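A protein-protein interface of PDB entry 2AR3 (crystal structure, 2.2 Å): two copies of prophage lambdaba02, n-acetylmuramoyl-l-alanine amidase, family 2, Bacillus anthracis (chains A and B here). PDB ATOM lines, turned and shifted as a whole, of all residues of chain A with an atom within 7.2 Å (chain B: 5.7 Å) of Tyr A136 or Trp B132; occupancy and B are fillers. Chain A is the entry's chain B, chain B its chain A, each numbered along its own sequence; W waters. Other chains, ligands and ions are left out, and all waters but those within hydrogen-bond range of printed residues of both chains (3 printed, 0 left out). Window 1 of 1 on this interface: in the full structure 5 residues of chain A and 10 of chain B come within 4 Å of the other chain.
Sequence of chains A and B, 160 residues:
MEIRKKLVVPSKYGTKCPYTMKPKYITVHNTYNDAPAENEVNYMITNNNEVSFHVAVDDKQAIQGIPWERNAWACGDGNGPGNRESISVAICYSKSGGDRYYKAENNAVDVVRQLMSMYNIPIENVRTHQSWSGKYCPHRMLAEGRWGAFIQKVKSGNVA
O of Ser A133 lies close to O of Ser B133 (3.4 Å).
The backbone NH (N) of Tyr A136 sits at hydrogen-bond distance from the backbone carbonyl oxygen (O) of Trp B132 (2.9 Å).
The side-chain hydroxyl of Ser A133 sits at hydrogen-bond distance from a ring nitrogen (NE2) of His A129 (3.2 Å).
The backbone carbonyl oxygen (O) of Thr B128 is in hydrogen-bond range of the side-chain hydroxyl (OG) of Ser B131 (2.9 Å).
A ring nitrogen (NE2) of His B129 is in hydrogen-bond range of the side-chain hydroxyl (OG) of Ser B133.
The side-chain carboxylate (OD2) of Asp B77 sits at hydrogen-bond distance from the backbone NH (N) of Gly B82 (2.8 Å).
The side-chain hydroxyl of Tyr A136 is in hydrogen-bond range of the backbone NH of Ala A143.
NE1 of Trp B132 sits at hydrogen-bond distance from OG1 of Thr B27 (2.9 Å).
Gly A134 touches Trp B132 (O to O, 3.7 Å).
C of Ser B133 touches O of Gly A134, at 3.3 Å.
O of Gly A134 touches N of Gly B134, 3.5 Å away.
Lys A135 touches Asp B77.
CA of Lys A135 touches O of Trp B132, at 3.4 Å.
Lys A135 touches Ser B133 (N to O, 3.9 Å).
O of Ser B131 touches CD1 of Tyr A136, at 3.6 Å.
Of chain B, only Ser B131 (3.6 Å) and Trp B132 (2.9 Å) come within 4 Å of Tyr A136.
Of chain A, only Gly A134, Lys A135 and Tyr A136 come within 4 Å of Trp B132.
Printed residues of chain B within 4 Å of Ser A133: Ser B133.
Of the printed residues of chain B, Gly A134 touches Trp B132 (3.7 Å), Ser B133 (3.3 Å) and Gly B134 (3.5 Å).
Of the printed residues of chain A, Ser B131 touches Tyr A136 (3.6 Å).
Of the printed residues of chain A, Ser B133 touches Ser A133, Gly A134 and Lys A135.
Of the printed residues of chain A, Gly B134 touches Gly A134.
Thr B27 touches none of the printed residues of chain A.
The nearest residue of chain B that does not touch Tyr A136 is Pro B81 (4.4 Å).
The nearest residue of chain A that does not touch Trp B132 is Cys A137 (5.9 Å).
The nearest printed residue of chain B that does not touch Lys A135 is Gly B134 (4.9 Å).
Printed residues of chain A that touch a printed residue of chain B: Ser A133, Gly A134, Lys A135 and Tyr A136.
Among the printed residues, no Asp or Glu carboxylate lies within 4 Å of a Lys or Arg side-chain nitrogen of the other chain.
Ser B133 touches its own counterpart, Ser A133.
Gly A134 touches Ser B133, but with the chains exchanged Ser A133 does not touch Gly B134 (4.9 Å).
Gly A134 touches its own counterpart, Gly B134.
Of the 9 pairs that touch across the chains among the printed residues, 2 have their exchanged pair printed and touching as well.
Water W2 bridges O of Ser A133 (2.6 Å) and O of Ser B133 (2.6 Å).
Water W3 lies within hydrogen-bond range of O of Gly A134 (2.6 Å), O of Ser B131 (2.8 Å), NE2 of Gln A130 (2.8 Å) and N of Tyr A136 (3.5 Å).
Water W1 lies within hydrogen-bond range of OH of Tyr A136 (3.1 Å) and NH1 of Arg B127 (3.2 Å).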
ATOM      1  N   ASN A  30     -21.036   9.402  -8.176  1.00  0.00           N
ATOM      2  CA  ASN A  30     -20.586   8.031  -8.473  1.00  0.00           C
ATOM      3  C   ASN A  30     -21.451   7.783  -9.703  1.00  0.00           C
ATOM      4  O   ASN A  30     -22.631   8.136  -9.706  1.00  0.00           O
ATOM      5  CB  ASN A  30     -20.984   7.026  -7.376  1.00  0.00           C
ATOM      6  CG  ASN A  30     -19.951   6.906  -6.262  1.00  0.00           C
ATOM      7  OD1 ASN A  30     -20.214   6.283  -5.241  1.00  0.00           O
ATOM      8  ND2 ASN A  30     -18.770   7.491  -6.461  1.00  0.00           N
ATOM      9  N   HIS A 129     -23.999  14.910  -4.349  1.00  0.00           N
ATOM     10  CA  HIS A 129     -25.095  15.171  -5.262  1.00  0.00           C
ATOM     11  C   HIS A 129     -26.367  15.201  -4.416  1.00  0.00           C
ATOM     12  O   HIS A 129     -27.232  16.052  -4.599  1.00  0.00           O
ATOM     13  CB  HIS A 129     -25.168  14.060  -6.323  1.00  0.00           C
ATOM     14  CG  HIS A 129     -26.347  14.162  -7.256  1.00  0.00           C
ATOM     15  ND1 HIS A 129     -26.526  13.303  -8.301  1.00  0.00           N
ATOM     16  CD2 HIS A 129     -27.408  15.014  -7.260  1.00  0.00           C
ATOM     17  CE1 HIS A 129     -27.666  13.607  -8.932  1.00  0.00           C
ATOM     18  NE2 HIS A 129     -28.206  14.627  -8.319  1.00  0.00           N
ATOM     19  N   GLN A 130     -26.458  14.273  -3.468  1.00  0.00           N
ATOM     20  CA  GLN A 130     -27.624  14.180  -2.599  1.00  0.00           C
ATOM     21  C   GLN A 130     -27.964  15.474  -1.851  1.00  0.00           C
ATOM     22  O   GLN A 130     -29.145  15.793  -1.663  1.00  0.00           O
ATOM     23  CB  GLN A 130     -27.426  13.055  -1.583  1.00  0.00           C
ATOM     24  CG  GLN A 130     -28.532  12.939  -0.532  1.00  0.00           C
ATOM     25  CD  GLN A 130     -28.174  11.941   0.554  1.00  0.00           C
ATOM     26  OE1 GLN A 130     -27.229  12.158   1.314  1.00  0.00           O
ATOM     27  NE2 GLN A 130     -28.910  10.831   0.620  1.00  0.00           N
ATOM     28  N   SER A 133     -30.222  17.746  -4.475  1.00  0.00           N
ATOM     29  CA  SER A 133     -31.522  17.297  -4.948  1.00  0.00           C
ATOM     30  C   SER A 133     -32.188  16.137  -4.207  1.00  0.00           C
ATOM     31  O   SER A 133     -33.340  15.825  -4.474  1.00  0.00           O
ATOM     32  CB  SER A 133     -31.409  16.932  -6.431  1.00  0.00           C
ATOM     33  OG  SER A 133     -30.652  15.736  -6.582  1.00  0.00           O
ATOM     34  N   GLY A 134     -31.485  15.497  -3.282  1.00  0.00           N
ATOM     35  CA  GLY A 134     -32.097  14.393  -2.571  1.00  0.00           C
ATOM     36  C   GLY A 134     -31.808  13.025  -3.163  1.00  0.00           C
ATOM     37  O   GLY A 134     -32.116  11.999  -2.549  1.00  0.00           O
ATOM     38  N   LYS A 135     -31.215  12.989  -4.354  1.00  0.00           N
ATOM     39  CA  LYS A 135     -30.893  11.707  -4.975  1.00  0.00           C
ATOM     40  C   LYS A 135     -29.800  11.004  -4.173  1.00  0.00           C
ATOM     41  O   LYS A 135     -28.920  11.654  -3.621  1.00  0.00           O
ATOM     42  CB  LYS A 135     -30.423  11.892  -6.420  1.00  0.00           C
ATOM     43  CG  LYS A 135     -30.174  10.570  -7.114  1.00  0.00           C
ATOM     44  CD  LYS A 135     -29.747  10.750  -8.552  1.00  0.00           C
ATOM     45  CE  LYS A 135     -29.416   9.410  -9.161  1.00  0.00           C
ATOM     46  NZ  LYS A 135     -29.037   9.553 -10.581  1.00  0.00           N
ATOM     47  N   TYR A 136     -29.862   9.678  -4.114  1.00  0.00           N
ATOM     48  CA  TYR A 136     -28.884   8.879  -3.363  1.00  0.00           C
ATOM     49  C   TYR A 136     -27.584   8.708  -4.169  1.00  0.00           C
ATOM     50  O   TYR A 136     -27.324   7.640  -4.711  1.00  0.00           O
ATOM     51  CB  TYR A 136     -29.507   7.505  -3.031  1.00  0.00           C
ATOM     52  CG  TYR A 136     -28.804   6.672  -1.961  1.00  0.00           C
ATOM     53  CD1 TYR A 136     -28.869   7.030  -0.621  1.00  0.00           C
ATOM     54  CD2 TYR A 136     -28.077   5.520  -2.297  1.00  0.00           C
ATOM     55  CE1 TYR A 136     -28.234   6.271   0.369  1.00  0.00           C
ATOM     56  CE2 TYR A 136     -27.430   4.746  -1.312  1.00  0.00           C
ATOM     57  CZ  TYR A 136     -27.513   5.134   0.021  1.00  0.00           C
ATOM     58  OH  TYR A 136     -26.864   4.419   1.010  1.00  0.00           O
ATOM     59  N   CYS A 137     -26.796   9.777  -4.250  1.00  0.00           N
ATOM     60  CA  CYS A 137     -25.521   9.784  -4.965  1.00  0.00           C
ATOM     61  C   CYS A 137     -24.502  10.654  -4.177  1.00  0.00           C
ATOM     62  O   CYS A 137     -24.844  11.743  -3.740  1.00  0.00           O
ATOM     63  CB  CYS A 137     -25.725  10.347  -6.348  1.00  0.00           C
ATOM     64  SG  CYS A 137     -24.108  10.775  -7.040  1.00  0.00           S
ATOM     65  N   PRO A 138     -23.227  10.218  -4.040  1.00  0.00           N
ATOM     66  CA  PRO A 138     -22.639   8.957  -4.497  1.00  0.00           C
ATOM     67  C   PRO A 138     -23.077   7.752  -3.697  1.00  0.00           C
ATOM     68  O   PRO A 138     -22.648   7.547  -2.554  1.00  0.00           O
ATOM     69  CB  PRO A 138     -21.145   9.231  -4.373  1.00  0.00           C
ATOM     70  CG  PRO A 138     -21.078  10.024  -3.122  1.00  0.00           C
ATOM     71  CD  PRO A 138     -22.249  10.966  -3.218  1.00  0.00           C
ATOM     72  N   HIS A 139     -23.902   6.926  -4.332  1.00  0.00           N
ATOM     73  CA  HIS A 139     -24.466   5.750  -3.685  1.00  0.00           C
ATOM     74  C   HIS A 139     -23.462   4.906  -2.902  1.00  0.00           C
ATOM     75  O   HIS A 139     -23.649   4.682  -1.710  1.00  0.00           O
ATOM     76  CB  HIS A 139     -25.196   4.888  -4.716  1.00  0.00           C
ATOM     77  CG  HIS A 139     -24.281   4.176  -5.658  1.00  0.00           C
ATOM     78  ND1 HIS A 139     -23.977   2.839  -5.527  1.00  0.00           N
ATOM     79  CD2 HIS A 139     -23.562   4.627  -6.711  1.00  0.00           C
ATOM     80  CE1 HIS A 139     -23.107   2.495  -6.457  1.00  0.00           C
ATOM     81  NE2 HIS A 139     -22.837   3.561  -7.189  1.00  0.00           N
ATOM     82  N   ARG A 140     -22.384   4.457  -3.538  1.00  0.00           N
ATOM     83  CA  ARG A 140     -21.432   3.621  -2.812  1.00  0.00           C
ATOM     84  C   ARG A 140     -20.763   4.336  -1.641  1.00  0.00           C
ATOM     85  O   ARG A 140     -20.611   3.748  -0.569  1.00  0.00           O
ATOM     86  CB  ARG A 140     -20.378   3.041  -3.746  1.00  0.00           C
ATOM     87  CG  ARG A 140     -19.442   2.050  -3.051  1.00  0.00           C
ATOM     88  CD  ARG A 140     -18.579   1.360  -4.085  1.00  0.00           C
ATOM     89  NE  ARG A 140     -19.352   0.391  -4.868  1.00  0.00           N
ATOM     90  CZ  ARG A 140     -19.723  -0.803  -4.408  1.00  0.00           C
ATOM     91  NH1 ARG A 140     -19.395  -1.185  -3.176  1.00  0.00           N
ATOM     92  NH2 ARG A 140     -20.412  -1.620  -5.178  1.00  0.00           N
ATOM     93  N   MET A 141     -20.362   5.592  -1.825  1.00  0.00           N
ATOM     94  CA  MET A 141     -19.739   6.340  -0.730  1.00  0.00           C
ATOM     95  C   MET A 141     -20.712   6.499   0.441  1.00  0.00           C
ATOM     96  O   MET A 141     -20.307   6.475   1.609  1.00  0.00           O
ATOM     97  CB  MET A 141     -19.295   7.723  -1.209  1.00  0.00           C
ATOM     98  CG  MET A 141     -18.205   7.684  -2.256  1.00  0.00           C
ATOM     99  SD  MET A 141     -17.583   9.352  -2.596  1.00  0.00           S
ATOM    100  CE  MET A 141     -16.790   9.731  -1.068  1.00  0.00           C
ATOM    101  N   LEU A 142     -21.991   6.669   0.114  1.00  0.00           N
ATOM    102  CA  LEU A 142     -23.044   6.822   1.111  1.00  0.00           C
ATOM    103  C   LEU A 142     -23.320   5.497   1.835  1.00  0.00           C
ATOM    104  O   LEU A 142     -23.291   5.436   3.057  1.00  0.00           O
ATOM    105  CB  LEU A 142     -24.331   7.341   0.436  1.00  0.00           C
ATOM    106  CG  LEU A 142     -24.296   8.768  -0.136  1.00  0.00           C
ATOM    107  CD1 LEU A 142     -25.572   9.088  -0.925  1.00  0.00           C
ATOM    108  CD2 LEU A 142     -24.144   9.749   1.012  1.00  0.00           C
ATOM    109  N   ALA A 143     -23.570   4.437   1.076  1.00  0.00           N
ATOM    110  CA  ALA A 143     -23.853   3.136   1.670  1.00  0.00           C
ATOM    111  C   ALA A 143     -22.689   2.608   2.515  1.00  0.00           C
ATOM    112  O   ALA A 143     -22.908   1.955   3.535  1.00  0.00           O
ATOM    113  CB  ALA A 143     -24.202   2.136   0.578  1.00  0.00           C
ATOM    114  N   GLU A 144     -21.459   2.888   2.096  1.00  0.00           N
ATOM    115  CA  GLU A 144     -20.291   2.426   2.834  1.00  0.00           C
ATOM    116  C   GLU A 144     -19.807   3.449   3.853  1.00  0.00           C
ATOM    117  O   GLU A 144     -18.837   3.215   4.572  1.00  0.00           O
ATOM    118  CB  GLU A 144     -19.175   2.051   1.859  1.00  0.00           C
ATOM    119  CG  GLU A 144     -19.376   0.685   1.233  1.00  0.00           C
ATOM    120  CD  GLU A 144     -18.382   0.403   0.132  1.00  0.00           C
ATOM    121  OE1 GLU A 144     -17.252   0.929   0.210  1.00  0.00           O
ATOM    122  OE2 GLU A 144     -18.721  -0.345  -0.812  1.00  0.00           O
ATOM    123  N   GLY A 145     -20.501   4.581   3.919  1.00  0.00           N
ATOM    124  CA  GLY A 145     -20.145   5.624   4.865  1.00  0.00           C
ATOM    125  C   GLY A 145     -18.722   6.126   4.719  1.00  0.00           C
ATOM    126  O   GLY A 145     -18.030   6.300   5.711  1.00  0.00           O
ATOM    127  N   TYR B  25     -32.997  -4.604  -2.946  1.00  0.00           N
ATOM    128  CA  TYR B  25     -33.764  -3.772  -2.024  1.00  0.00           C
ATOM    129  C   TYR B  25     -35.261  -3.853  -2.313  1.00  0.00           C
ATOM    130  O   TYR B  25     -35.706  -4.269  -3.392  1.00  0.00           O
ATOM    131  CB  TYR B  25     -33.370  -2.294  -2.131  1.00  0.00           C
ATOM    132  CG  TYR B  25     -31.893  -2.032  -2.209  1.00  0.00           C
ATOM    133  CD1 TYR B  25     -31.150  -1.730  -1.067  1.00  0.00           C
ATOM    134  CD2 TYR B  25     -31.234  -2.092  -3.431  1.00  0.00           C
ATOM    135  CE1 TYR B  25     -29.786  -1.495  -1.146  1.00  0.00           C
ATOM    136  CE2 TYR B  25     -29.874  -1.861  -3.524  1.00  0.00           C
ATOM    137  CZ  TYR B  25     -29.156  -1.564  -2.383  1.00  0.00           C
ATOM    138  OH  TYR B  25     -27.803  -1.344  -2.459  1.00  0.00           O
ATOM    139  N   ILE B  26     -36.031  -3.430  -1.321  1.00  0.00           N
ATOM    140  CA  ILE B  26     -37.476  -3.369  -1.424  1.00  0.00           C
ATOM    141  C   ILE B  26     -37.762  -1.914  -1.085  1.00  0.00           C
ATOM    142  O   ILE B  26     -37.272  -1.407  -0.073  1.00  0.00           O
ATOM    143  CB  ILE B  26     -38.167  -4.281  -0.388  1.00  0.00           C
ATOM    144  CG1 ILE B  26     -37.806  -5.746  -0.658  1.00  0.00           C
ATOM    145  CG2 ILE B  26     -39.679  -4.055  -0.435  1.00  0.00           C
ATOM    146  CD1 ILE B  26     -38.129  -6.661   0.500  1.00  0.00           C
ATOM    147  N   THR B  27     -38.510  -1.230  -1.948  1.00  0.00           N
ATOM    148  CA  THR B  27     -38.848   0.175  -1.729  1.00  0.00           C
ATOM    149  C   THR B  27     -40.337   0.292  -1.474  1.00  0.00           C
ATOM    150  O   THR B  27     -41.131  -0.181  -2.267  1.00  0.00           O
ATOM    151  CB  THR B  27     -38.509   1.041  -2.958  1.00  0.00           C
ATOM    152  OG1 THR B  27     -37.098   0.952  -3.236  1.00  0.00           O
ATOM    153  CG2 THR B  27     -38.943   2.527  -2.710  1.00  0.00           C
ATOM    154  N   CYS B  75     -38.906   5.062  -8.410  1.00  0.00           N
ATOM    155  CA  CYS B  75     -38.066   5.751  -7.427  1.00  0.00           C
ATOM    156  C   CYS B  75     -37.545   7.129  -7.850  1.00  0.00           C
ATOM    157  O   CYS B  75     -36.920   7.834  -7.055  1.00  0.00           O
ATOM    158  CB  CYS B  75     -36.899   4.830  -7.050  1.00  0.00           C
ATOM    159  SG  CYS B  75     -37.434   3.217  -6.353  1.00  0.00           S
ATOM    160  N   ASP B  77     -35.076   8.048  -9.339  1.00  0.00           N
ATOM    161  CA  ASP B  77     -33.636   8.243  -9.231  1.00  0.00           C
ATOM    162  C   ASP B  77     -32.991   7.812 -10.547  1.00  0.00           C
ATOM    163  O   ASP B  77     -31.854   7.331 -10.579  1.00  0.00           O
ATOM    164  CB  ASP B  77     -33.066   7.429  -8.061  1.00  0.00           C
ATOM    165  CG  ASP B  77     -33.073   5.921  -8.324  1.00  0.00           C
ATOM    166  OD1 ASP B  77     -33.933   5.452  -9.103  1.00  0.00           O
ATOM    167  OD2 ASP B  77     -32.216   5.213  -7.737  1.00  0.00           O
ATOM    168  N   PRO B  81     -29.636   2.853  -8.006  1.00  0.00           N
ATOM    169  CA  PRO B  81     -29.992   1.596  -7.334  1.00  0.00           C
ATOM    170  C   PRO B  81     -31.480   1.463  -7.009  1.00  0.00           C
ATOM    171  O   PRO B  81     -32.024   0.354  -6.963  1.00  0.00           O
ATOM    172  CB  PRO B  81     -29.123   1.620  -6.077  1.00  0.00           C
ATOM    173  CG  PRO B  81     -28.993   3.093  -5.793  1.00  0.00           C
ATOM    174  CD  PRO B  81     -28.722   3.648  -7.167  1.00  0.00           C
ATOM    175  N   GLY B  82     -32.128   2.598  -6.764  1.00  0.00           N
ATOM    176  CA  GLY B  82     -33.549   2.577  -6.469  1.00  0.00           C
ATOM    177  C   GLY B  82     -34.342   1.959  -7.609  1.00  0.00           C
ATOM    178  O   GLY B  82     -35.029   0.955  -7.423  1.00  0.00           O
ATOM    179  N   SER B  86     -34.275  -2.321  -6.788  1.00  0.00           N
ATOM    180  CA  SER B  86     -35.289  -2.532  -5.777  1.00  0.00           C
ATOM    181  C   SER B  86     -36.646  -2.845  -6.383  1.00  0.00           C
ATOM    182  O   SER B  86     -36.970  -2.444  -7.516  1.00  0.00           O
ATOM    183  CB  SER B  86     -35.395  -1.327  -4.829  1.00  0.00           C
ATOM    184  OG  SER B  86     -36.224  -0.314  -5.375  1.00  0.00           O
ATOM    185  N   ARG B 127     -36.392  -0.028   2.055  1.00  0.00           N
ATOM    186  CA  ARG B 127     -36.284   1.418   2.042  1.00  0.00           C
ATOM    187  C   ARG B 127     -37.556   2.153   1.638  1.00  0.00           C
ATOM    188  O   ARG B 127     -38.538   1.548   1.178  1.00  0.00           O
ATOM    189  CB  ARG B 127     -35.135   1.823   1.101  1.00  0.00           C
ATOM    190  CG  ARG B 127     -33.819   1.054   1.318  1.00  0.00           C
ATOM    191  CD  ARG B 127     -33.152   1.384   2.647  1.00  0.00           C
ATOM    192  NE  ARG B 127     -31.990   0.527   2.889  1.00  0.00           N
ATOM    193  CZ  ARG B 127     -30.809   0.649   2.281  1.00  0.00           C
ATOM    194  NH1 ARG B 127     -30.612   1.607   1.383  1.00  0.00           N
ATOM    195  NH2 ARG B 127     -29.820  -0.197   2.557  1.00  0.00           N
ATOM    196  N   THR B 128     -37.519   3.470   1.822  1.00  0.00           N
ATOM    197  CA  THR B 128     -38.622   4.350   1.478  1.00  0.00           C
ATOM    198  C   THR B 128     -38.245   4.956   0.141  1.00  0.00           C
ATOM    199  O   THR B 128     -37.069   4.925  -0.243  1.00  0.00           O
ATOM    200  CB  THR B 128     -38.729   5.522   2.461  1.00  0.00           C
ATOM    201  OG1 THR B 128     -37.528   6.303   2.380  1.00  0.00           O
ATOM    202  CG2 THR B 128     -38.926   5.029   3.900  1.00  0.00           C
ATOM    203  N   HIS B 129     -39.235   5.505  -0.564  1.00  0.00           N
ATOM    204  CA  HIS B 129     -38.988   6.157  -1.853  1.00  0.00           C
ATOM    205  C   HIS B 129     -38.133   7.396  -1.565  1.00  0.00           C
ATOM    206  O   HIS B 129     -37.187   7.706  -2.289  1.00  0.00           O
ATOM    207  CB  HIS B 129     -40.317   6.575  -2.507  1.00  0.00           C
ATOM    208  CG  HIS B 129     -40.174   7.325  -3.801  1.00  0.00           C
ATOM    209  ND1 HIS B 129     -41.263   7.698  -4.556  1.00  0.00           N
ATOM    210  CD2 HIS B 129     -39.084   7.815  -4.450  1.00  0.00           C
ATOM    211  CE1 HIS B 129     -40.855   8.387  -5.611  1.00  0.00           C
ATOM    212  NE2 HIS B 129     -39.541   8.471  -5.567  1.00  0.00           N
ATOM    213  N   GLN B 130     -38.468   8.090  -0.486  1.00  0.00           N
ATOM    214  CA  GLN B 130     -37.736   9.291  -0.092  1.00  0.00           C
ATOM    215  C   GLN B 130     -36.228   9.076   0.009  1.00  0.00           C
ATOM    216  O   GLN B 130     -35.452   9.948  -0.388  1.00  0.00           O
ATOM    217  CB  GLN B 130     -38.262   9.794   1.247  1.00  0.00           C
ATOM    218  CG  GLN B 130     -37.561  11.031   1.784  1.00  0.00           C
ATOM    219  CD  GLN B 130     -38.130  11.457   3.118  1.00  0.00           C
ATOM    220  OE1 GLN B 130     -38.211  10.652   4.048  1.00  0.00           O
ATOM    221  NE2 GLN B 130     -38.534  12.724   3.221  1.00  0.00           N
ATOM    222  N   SER B 131     -35.809   7.919   0.521  1.00  0.00           N
ATOM    223  CA  SER B 131     -34.384   7.642   0.688  1.00  0.00           C
ATOM    224  C   SER B 131     -33.617   7.558  -0.632  1.00  0.00           C
ATOM    225  O   SER B 131     -32.393   7.704  -0.650  1.00  0.00           O
ATOM    226  CB  SER B 131     -34.176   6.351   1.504  1.00  0.00           C
ATOM    227  OG  SER B 131     -34.331   5.181   0.710  1.00  0.00           O
ATOM    228  N   TRP B 132     -34.327   7.340  -1.737  1.00  0.00           N
ATOM    229  CA  TRP B 132     -33.667   7.253  -3.042  1.00  0.00           C
ATOM    230  C   TRP B 132     -33.617   8.563  -3.814  1.00  0.00           C
ATOM    231  O   TRP B 132     -32.621   8.850  -4.468  1.00  0.00           O
ATOM    232  CB  TRP B 132     -34.349   6.221  -3.945  1.00  0.00           C
ATOM    233  CG  TRP B 132     -34.281   4.830  -3.474  1.00  0.00           C
ATOM    234  CD1 TRP B 132     -35.336   4.000  -3.237  1.00  0.00           C
ATOM    235  CD2 TRP B 132     -33.102   4.061  -3.202  1.00  0.00           C
ATOM    236  NE1 TRP B 132     -34.891   2.764  -2.833  1.00  0.00           N
ATOM    237  CE2 TRP B 132     -33.515   2.773  -2.805  1.00  0.00           C
ATOM    238  CE3 TRP B 132     -31.730   4.339  -3.254  1.00  0.00           C
ATOM    239  CZ2 TRP B 132     -32.621   1.755  -2.466  1.00  0.00           C
ATOM    240  CZ3 TRP B 132     -30.823   3.329  -2.915  1.00  0.00           C
ATOM    241  CH2 TRP B 132     -31.276   2.047  -2.524  1.00  0.00           C
ATOM    242  N   SER B 133     -34.682   9.360  -3.751  1.00  0.00           N
ATOM    243  CA  SER B 133     -34.712  10.600  -4.531  1.00  0.00           C
ATOM    244  C   SER B 133     -35.168  11.851  -3.794  1.00  0.00           C
ATOM    245  O   SER B 133     -35.116  12.951  -4.349  1.00  0.00           O
ATOM    246  CB  SER B 133     -35.594  10.404  -5.764  1.00  0.00           C
ATOM    247  OG  SER B 133     -36.918  10.100  -5.366  1.00  0.00           O
ATOM    248  N   GLY B 134     -35.609  11.683  -2.551  1.00  0.00           N
ATOM    249  CA  GLY B 134     -36.058  12.826  -1.778  1.00  0.00           C
ATOM    250  C   GLY B 134     -37.553  13.090  -1.772  1.00  0.00           C
ATOM    251  O   GLY B 134     -38.026  13.889  -0.963  1.00  0.00           O
HETATM  252  O   HOH W   1     -27.685   1.589   0.200  1.00  0.00           O
HETATM  253  O   HOH W   2     -35.344  15.011  -5.964  1.00  0.00           O
HETATM  254  O   HOH W   3     -31.172  10.164  -0.913  1.00  0.00           O
